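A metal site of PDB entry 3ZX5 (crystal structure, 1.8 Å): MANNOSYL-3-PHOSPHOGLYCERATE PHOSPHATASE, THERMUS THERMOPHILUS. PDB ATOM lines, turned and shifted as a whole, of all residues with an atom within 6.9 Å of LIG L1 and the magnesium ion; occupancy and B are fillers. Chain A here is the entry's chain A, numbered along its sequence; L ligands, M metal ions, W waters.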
ATOM      1  N   THR A   5      -1.218  13.167  -3.715  1.00  0.00           N
ATOM      2  CA  THR A   5      -0.258  13.737  -2.766  1.00  0.00           C
ATOM      3  C   THR A   5      -0.239  13.068  -1.400  1.00  0.00           C
ATOM      4  O   THR A   5      -1.272  12.783  -0.824  1.00  0.00           O
ATOM      5  CB  THR A   5      -0.464  15.251  -2.592  1.00  0.00           C
ATOM      6  OG1 THR A   5       0.525  15.765  -1.679  1.00  0.00           O
ATOM      7  CG2 THR A   5      -1.850  15.560  -2.046  1.00  0.00           C
ATOM      8  N   ASP A   6       0.973  12.829  -0.907  1.00  0.00           N
ATOM      9  CA  ASP A   6       1.196  12.390   0.444  1.00  0.00           C
ATOM     10  C   ASP A   6       0.811  13.550   1.373  1.00  0.00           C
ATOM     11  O   ASP A   6       0.739  14.702   0.931  1.00  0.00           O
ATOM     12  CB  ASP A   6       2.666  12.018   0.589  1.00  0.00           C
ATOM     13  CG  ASP A   6       3.071  11.738   1.999  1.00  0.00           C
ATOM     14  OD1 ASP A   6       2.411  10.950   2.704  1.00  0.00           O
ATOM     15  OD2 ASP A   6       4.080  12.340   2.401  1.00  0.00           O
ATOM     16  N   LEU A   7       0.554  13.243   2.632  1.00  0.00           N
ATOM     17  CA  LEU A   7       0.157  14.284   3.587  1.00  0.00           C
ATOM     18  C   LEU A   7       1.314  14.723   4.478  1.00  0.00           C
ATOM     19  O   LEU A   7       1.902  15.776   4.245  1.00  0.00           O
ATOM     20  CB  LEU A   7      -1.044  13.821   4.419  1.00  0.00           C
ATOM     21  CG  LEU A   7      -2.269  13.480   3.569  1.00  0.00           C
ATOM     22  CD1 LEU A   7      -3.409  12.982   4.438  1.00  0.00           C
ATOM     23  CD2 LEU A   7      -2.716  14.686   2.736  1.00  0.00           C
ATOM     24  N   ASP A   8       1.647  13.907   5.498  1.00  0.00           N
ATOM     25  CA  ASP A   8       2.712  14.280   6.440  1.00  0.00           C
ATOM     26  C   ASP A   8       3.983  14.665   5.694  1.00  0.00           C
ATOM     27  O   ASP A   8       4.477  13.902   4.892  1.00  0.00           O
ATOM     28  CB  ASP A   8       3.050  13.107   7.363  1.00  0.00           C
ATOM     29  CG  ASP A   8       1.936  12.805   8.352  1.00  0.00           C
ATOM     30  OD1 ASP A   8       1.285  13.753   8.836  1.00  0.00           O
ATOM     31  OD2 ASP A   8       1.722  11.608   8.641  1.00  0.00           O
ATOM     32  N   GLY A   9       4.495  15.848   5.965  1.00  0.00           N
ATOM     33  CA  GLY A   9       5.788  16.227   5.425  1.00  0.00           C
ATOM     34  C   GLY A   9       5.778  16.589   3.955  1.00  0.00           C
ATOM     35  O   GLY A   9       6.825  16.889   3.389  1.00  0.00           O
ATOM     36  N   THR A  10       4.600  16.548   3.342  1.00  0.00           N
ATOM     37  CA  THR A  10       4.419  16.941   1.950  1.00  0.00           C
ATOM     38  C   THR A  10       3.361  18.038   1.849  1.00  0.00           C
ATOM     39  O   THR A  10       3.690  19.210   1.658  1.00  0.00           O
ATOM     40  CB  THR A  10       4.039  15.743   1.076  1.00  0.00           C
ATOM     41  OG1 THR A  10       5.073  14.751   1.150  1.00  0.00           O
ATOM     42  CG2 THR A  10       3.847  16.168  -0.368  1.00  0.00           C
ATOM     43  N   LEU A  11       2.095  17.670   1.986  1.00  0.00           N
ATOM     44  CA  LEU A  11       1.002  18.643   1.973  1.00  0.00           C
ATOM     45  C   LEU A  11       0.838  19.315   3.333  1.00  0.00           C
ATOM     46  O   LEU A  11       0.348  20.438   3.422  1.00  0.00           O
ATOM     47  CB  LEU A  11      -0.318  17.992   1.560  1.00  0.00           C
ATOM     48  CG  LEU A  11      -1.458  18.981   1.249  1.00  0.00           C
ATOM     49  CD1 LEU A  11      -1.172  19.716  -0.051  1.00  0.00           C
ATOM     50  CD2 LEU A  11      -2.830  18.295   1.165  1.00  0.00           C
ATOM     51  N   LEU A  12       1.244  18.626   4.388  1.00  0.00           N
ATOM     52  CA  LEU A  12       1.036  19.125   5.740  1.00  0.00           C
ATOM     53  C   LEU A  12       2.327  19.612   6.369  1.00  0.00           C
ATOM     54  O   LEU A  12       3.394  19.062   6.088  1.00  0.00           O
ATOM     55  CB  LEU A  12       0.408  18.047   6.629  1.00  0.00           C
ATOM     56  CG  LEU A  12      -0.954  17.510   6.178  1.00  0.00           C
ATOM     57  CD1 LEU A  12      -1.438  16.438   7.141  1.00  0.00           C
ATOM     58  CD2 LEU A  12      -1.960  18.645   6.071  1.00  0.00           C
ATOM     59  N   VAL A  38      -2.872  10.552  -0.704  1.00  0.00           N
ATOM     60  CA  VAL A  38      -2.358   9.177  -0.672  1.00  0.00           C
ATOM     61  C   VAL A  38      -1.374   9.066   0.492  1.00  0.00           C
ATOM     62  O   VAL A  38      -0.238   9.537   0.411  1.00  0.00           O
ATOM     63  CB  VAL A  38      -1.641   8.777  -1.975  1.00  0.00           C
ATOM     64  CG1 VAL A  38      -1.357   7.268  -1.985  1.00  0.00           C
ATOM     65  CG2 VAL A  38      -2.493   9.157  -3.191  1.00  0.00           C
ATOM     66  N   THR A  39      -1.809   8.402   1.565  1.00  0.00           N
ATOM     67  CA  THR A  39      -1.191   8.609   2.858  1.00  0.00           C
ATOM     68  C   THR A  39      -1.107   7.320   3.699  1.00  0.00           C
ATOM     69  O   THR A  39      -1.852   6.357   3.448  1.00  0.00           O
ATOM     70  CB  THR A  39      -1.974   9.726   3.615  1.00  0.00           C
ATOM     71  OG1 THR A  39      -1.386   9.978   4.904  1.00  0.00           O
ATOM     72  CG2 THR A  39      -3.428   9.320   3.815  1.00  0.00           C
ATOM     73  N   ALA A  40      -0.187   7.291   4.643  1.00  0.00           N
ATOM     74  CA  ALA A  40      -0.143   6.230   5.655  1.00  0.00           C
ATOM     75  C   ALA A  40      -1.251   6.438   6.676  1.00  0.00           C
ATOM     76  O   ALA A  40      -1.584   5.530   7.453  1.00  0.00           O
ATOM     77  CB  ALA A  40       1.233   6.216   6.365  1.00  0.00           C
ATOM     78  N   LYS A  41      -1.834   7.630   6.683  1.00  0.00           N
ATOM     79  CA  LYS A  41      -2.860   7.952   7.675  1.00  0.00           C
ATOM     80  C   LYS A  41      -4.140   7.128   7.487  1.00  0.00           C
ATOM     81  O   LYS A  41      -4.403   6.598   6.404  1.00  0.00           O
ATOM     82  CB  LYS A  41      -3.173   9.469   7.661  1.00  0.00           C
ATOM     83  CG  LYS A  41      -2.019  10.334   8.181  1.00  0.00           C
ATOM     84  CD  LYS A  41      -2.258  11.827   7.973  1.00  0.00           C
ATOM     85  CE  LYS A  41      -2.151  12.622   9.273  1.00  0.00           C
ATOM     86  NZ  LYS A  41      -0.816  12.444   9.957  1.00  0.00           N
ATOM     87  N   ASN A  59      -1.241   3.662   3.425  1.00  0.00           N
ATOM     88  CA  ASN A  59      -0.177   3.295   2.496  1.00  0.00           C
ATOM     89  C   ASN A  59      -0.671   2.535   1.274  1.00  0.00           C
ATOM     90  O   ASN A  59       0.075   1.773   0.653  1.00  0.00           O
ATOM     91  CB  ASN A  59       0.933   2.484   3.206  1.00  0.00           C
ATOM     92  CG  ASN A  59       1.853   3.362   4.025  1.00  0.00           C
ATOM     93  OD1 ASN A  59       2.061   4.530   3.686  1.00  0.00           O
ATOM     94  ND2 ASN A  59       2.407   2.810   5.109  1.00  0.00           N
ATOM     95  N   GLY A 165       7.391   5.680   6.849  1.00  0.00           N
ATOM     96  CA  GLY A 165       6.995   7.031   6.503  1.00  0.00           C
ATOM     97  C   GLY A 165       8.042   7.997   7.013  1.00  0.00           C
ATOM     98  O   GLY A 165       9.228   7.670   7.031  1.00  0.00           O
ATOM     99  N   GLY A 166       7.613   9.166   7.470  1.00  0.00           N
ATOM    100  CA  GLY A 166       8.574  10.152   7.918  1.00  0.00           C
ATOM    101  C   GLY A 166       9.312   9.698   9.166  1.00  0.00           C
ATOM    102  O   GLY A 166      10.512   9.967   9.332  1.00  0.00           O
ATOM    103  N   HIS A 170       6.216   0.577   9.180  1.00  0.00           N
ATOM    104  CA  HIS A 170       4.864   0.041   9.052  1.00  0.00           C
ATOM    105  C   HIS A 170       4.928  -1.416   8.632  1.00  0.00           C
ATOM    106  O   HIS A 170       5.878  -1.831   7.978  1.00  0.00           O
ATOM    107  CB  HIS A 170       4.068   0.820   8.001  1.00  0.00           C
ATOM    108  CG  HIS A 170       3.778   2.238   8.397  1.00  0.00           C
ATOM    109  ND1 HIS A 170       2.564   2.645   8.886  1.00  0.00           N
ATOM    110  CD2 HIS A 170       4.568   3.344   8.399  1.00  0.00           C
ATOM    111  CE1 HIS A 170       2.596   3.936   9.166  1.00  0.00           C
ATOM    112  NE2 HIS A 170       3.806   4.385   8.868  1.00  0.00           N
ATOM    113  N   LYS A 177       1.352   2.300  -2.193  1.00  0.00           N
ATOM    114  CA  LYS A 177       0.768   3.535  -2.713  1.00  0.00           C
ATOM    115  C   LYS A 177       0.636   3.496  -4.234  1.00  0.00           C
ATOM    116  O   LYS A 177      -0.340   4.006  -4.783  1.00  0.00           O
ATOM    117  CB  LYS A 177       1.575   4.765  -2.276  1.00  0.00           C
ATOM    118  CG  LYS A 177       1.450   5.087  -0.774  1.00  0.00           C
ATOM    119  CD  LYS A 177       1.981   6.475  -0.437  1.00  0.00           C
ATOM    120  CE  LYS A 177       1.738   6.818   1.056  1.00  0.00           C
ATOM    121  NZ  LYS A 177       2.217   8.168   1.397  1.00  0.00           N
ATOM    122  N   GLY A 201       5.627  13.610  -2.718  1.00  0.00           N
ATOM    123  CA  GLY A 201       5.913  12.920  -1.467  1.00  0.00           C
ATOM    124  C   GLY A 201       7.302  13.212  -0.948  1.00  0.00           C
ATOM    125  O   GLY A 201       8.066  13.970  -1.560  1.00  0.00           O
ATOM    126  N   ASP A 202       7.644  12.605   0.197  1.00  0.00           N
ATOM    127  CA  ASP A 202       8.886  12.949   0.891  1.00  0.00           C
ATOM    128  C   ASP A 202       9.641  11.797   1.564  1.00  0.00           C
ATOM    129  O   ASP A 202      10.712  12.020   2.107  1.00  0.00           O
ATOM    130  CB  ASP A 202       8.626  14.015   1.951  1.00  0.00           C
ATOM    131  CG  ASP A 202       7.802  13.496   3.115  1.00  0.00           C
ATOM    132  OD1 ASP A 202       6.618  13.203   2.905  1.00  0.00           O
ATOM    133  OD2 ASP A 202       8.327  13.361   4.244  1.00  0.00           O
ATOM    134  N   SER A 203       9.102  10.585   1.560  1.00  0.00           N
ATOM    135  CA  SER A 203       9.749   9.503   2.299  1.00  0.00           C
ATOM    136  C   SER A 203       9.715   8.183   1.556  1.00  0.00           C
ATOM    137  O   SER A 203       9.236   8.095   0.430  1.00  0.00           O
ATOM    138  CB  SER A 203       9.108   9.326   3.675  1.00  0.00           C
ATOM    139  OG  SER A 203       9.178  10.506   4.441  1.00  0.00           O
ATOM    140  N   ASN A 205       7.943   5.503   1.855  1.00  0.00           N
ATOM    141  CA  ASN A 205       6.650   4.963   1.483  1.00  0.00           C
ATOM    142  C   ASN A 205       6.055   5.657   0.250  1.00  0.00           C
ATOM    143  O   ASN A 205       5.033   5.227  -0.280  1.00  0.00           O
ATOM    144  CB  ASN A 205       5.659   4.967   2.667  1.00  0.00           C
ATOM    145  CG  ASN A 205       5.349   6.363   3.173  1.00  0.00           C
ATOM    146  OD1 ASN A 205       6.147   7.283   3.044  1.00  0.00           O
ATOM    147  ND2 ASN A 205       4.160   6.522   3.776  1.00  0.00           N
ATOM    148  N   ASP A 206       6.724   6.714  -0.208  1.00  0.00           N
ATOM    149  CA  ASP A 206       6.295   7.456  -1.410  1.00  0.00           C
ATOM    150  C   ASP A 206       6.954   6.988  -2.714  1.00  0.00           C
ATOM    151  O   ASP A 206       6.546   7.421  -3.814  1.00  0.00           O
ATOM    152  CB  ASP A 206       6.521   8.965  -1.221  1.00  0.00           C
ATOM    153  CG  ASP A 206       5.692   9.550  -0.090  1.00  0.00           C
ATOM    154  OD1 ASP A 206       4.508   9.184   0.051  1.00  0.00           O
ATOM    155  OD2 ASP A 206       6.198  10.416   0.652  1.00  0.00           O
HETATM  156  V1  LIG L   1       2.229  10.261   4.620  1.00  0.00           V
HETATM  157  O1  LIG L   1       2.166   8.422   4.159  1.00  0.00           O
HETATM  158  O2  LIG L   1       0.710  11.253   5.117  1.00  0.00           O
HETATM  159  O3  LIG L   1       3.906  10.846   5.288  1.00  0.00           O
HETATM  160  C1  LG2 L   2       2.276   7.345  10.844  1.00  0.00           C
HETATM  161  O1  LG2 L   2       2.449   7.793   9.497  1.00  0.00           O
HETATM  162  C2  LG2 L   2       3.599   8.619   9.263  1.00  0.00           C
HETATM  163  C3  LG2 L   2       3.584   9.048   7.781  1.00  0.00           C
HETATM  164  O2  LG2 L   2       4.759   9.801   7.479  1.00  0.00           O
HETATM  165  C4  LG2 L   2       4.881   7.907   9.608  1.00  0.00           C
HETATM  166  O3  LG2 L   2       5.082   6.743   9.195  1.00  0.00           O
HETATM  167  O4  LG2 L   2       5.829   8.601  10.037  1.00  0.00           O
HETATM  168  C5  LG2 L   2       0.878   6.744  10.972  1.00  0.00           C
HETATM  169  O5  LG2 L   2       0.711   6.108  12.255  1.00  0.00           O
HETATM  170  C6  LG2 L   2      -0.177   7.843  10.804  1.00  0.00           C
HETATM  171  O6  LG2 L   2      -1.472   7.288  10.974  1.00  0.00           O
HETATM  172  C7  LG2 L   2       0.072   8.914  11.851  1.00  0.00           C
HETATM  173  O7  LG2 L   2      -0.804  10.021  11.637  1.00  0.00           O
HETATM  174  C8  LG2 L   2       1.483   9.453  11.784  1.00  0.00           C
HETATM  175  C9  LG2 L   2       1.716  10.401  12.970  1.00  0.00           C
HETATM  176  O8  LG2 L   2       2.903  11.168  12.722  1.00  0.00           O
HETATM  177  O9  LG2 L   2       2.479   8.420  11.760  1.00  0.00           O
HETATM  178 MG    MG M   1       5.267  12.005   4.098  1.00  0.00          MG
HETATM  179  O   HOH W   1       6.693  11.951   5.780  1.00  0.00           O
HETATM  180  O   HOH W   2       5.876  10.026   3.173  1.00  0.00           O
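A vanadium atom (V1) of LIG L1 is bound by the side-chain carboxylate of Asp 6, 2.0 Å away. The side-chain hydroxyl (OG1) of Thr 39 sits close to an oxygen (O2) of LIG L1 (2.5 Å). An oxygen (O1) of LIG L1 lies close to the backbone NH (N) of Ala 40 (2.7 Å). The side-chain amino group of Lys 41 lies within hydrogen-bond range of an oxygen (O7) of LG2 L2 (2.9 Å). N of Gly 166 is in hydrogen-bond range of O2 of LG2 L2, at 2.9 Å. O3 of LG2 L2 sits close to N of Gly 165. A ring nitrogen (NE2) of His 170 sits at hydrogen-bond distance from an oxygen (O3) of LG2 L2 (2.7 Å).
An oxygen (O3) of LIG L1 lies close to an oxygen (O2) of LG2 L2 (2.6 Å).
The side-chain carboxylate (OD2) of Asp 6 sits close to the side-chain hydroxyl (OG1) of Thr 10. The backbone NH of Asp 202 lies within hydrogen-bond range of the side-chain hydroxyl of Thr 10 (3.5 Å). OG of Ser 203 lies within hydrogen-bond range of OD2 of Asp 202 (3.0 Å). NZ of Lys 41 lies within salt-bridge range of OD1 of Asp 8 (2.7 Å). NZ of Lys 177 sits close to ND2 of Asn 205 (3.5 Å). The backbone NH of Lys 177 sits at hydrogen-bond distance from the backbone carbonyl oxygen of Asn 59 (3.2 Å). The backbone carbonyl oxygen (O) of Leu 7 sits at hydrogen-bond distance from the backbone NH (N) of Leu 12 (2.9 Å). OD2 of Asp 206 sits at hydrogen-bond distance from N of Ser 203, 3.0 Å away.
N of Leu 7 lies close to O2 of LIG L1. An oxygen (O1) of LIG L1 sits close to the side-chain amino group (NZ) of Lys 177 (2.8 Å). An oxygen (O1) of LIG L1 sits close to the side-chain amide nitrogen (ND2) of Asn 205, 2.8 Å away. Residues that only touch LIG L1: Asn 59. Hydrophobic or aromatic side chains that line LIG L1: Leu 7 and Ala 40.
Asp 206 touches the magnesium ion (OD2 to MG, 3.9 Å).
OD2 of Asp 6 binds the magnesium ion, 2.1 Å away. O3 of LIG L1 is bound to the magnesium ion (2.1 Å). The magnesium ion is bound by the side-chain carboxylate (OD1) of Asp 202 (2.2 Å). The magnesium ion is bound by the backbone carbonyl oxygen (O) of Asp 8 (2.2 Å). Water W1 is bound to the magnesium ion. Water W2 is bound to the magnesium ion (2.3 Å). The magnesium ion has six donor atoms within binding distance.
Water W1 lies within hydrogen-bond range of the side-chain carboxylate of Asp 202 (2.6 Å), the side-chain hydroxyl of Ser 203 (3.2 Å), an oxygen (O2) of LG2 L2 (3.4 Å) and the backbone NH of Gly 166 (3.4 Å). Water W2 lies within hydrogen-bond range of the side-chain carboxylate of Asp 206 (2.6 Å) and the side-chain amide oxygen of Asn 205 (2.8 Å).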
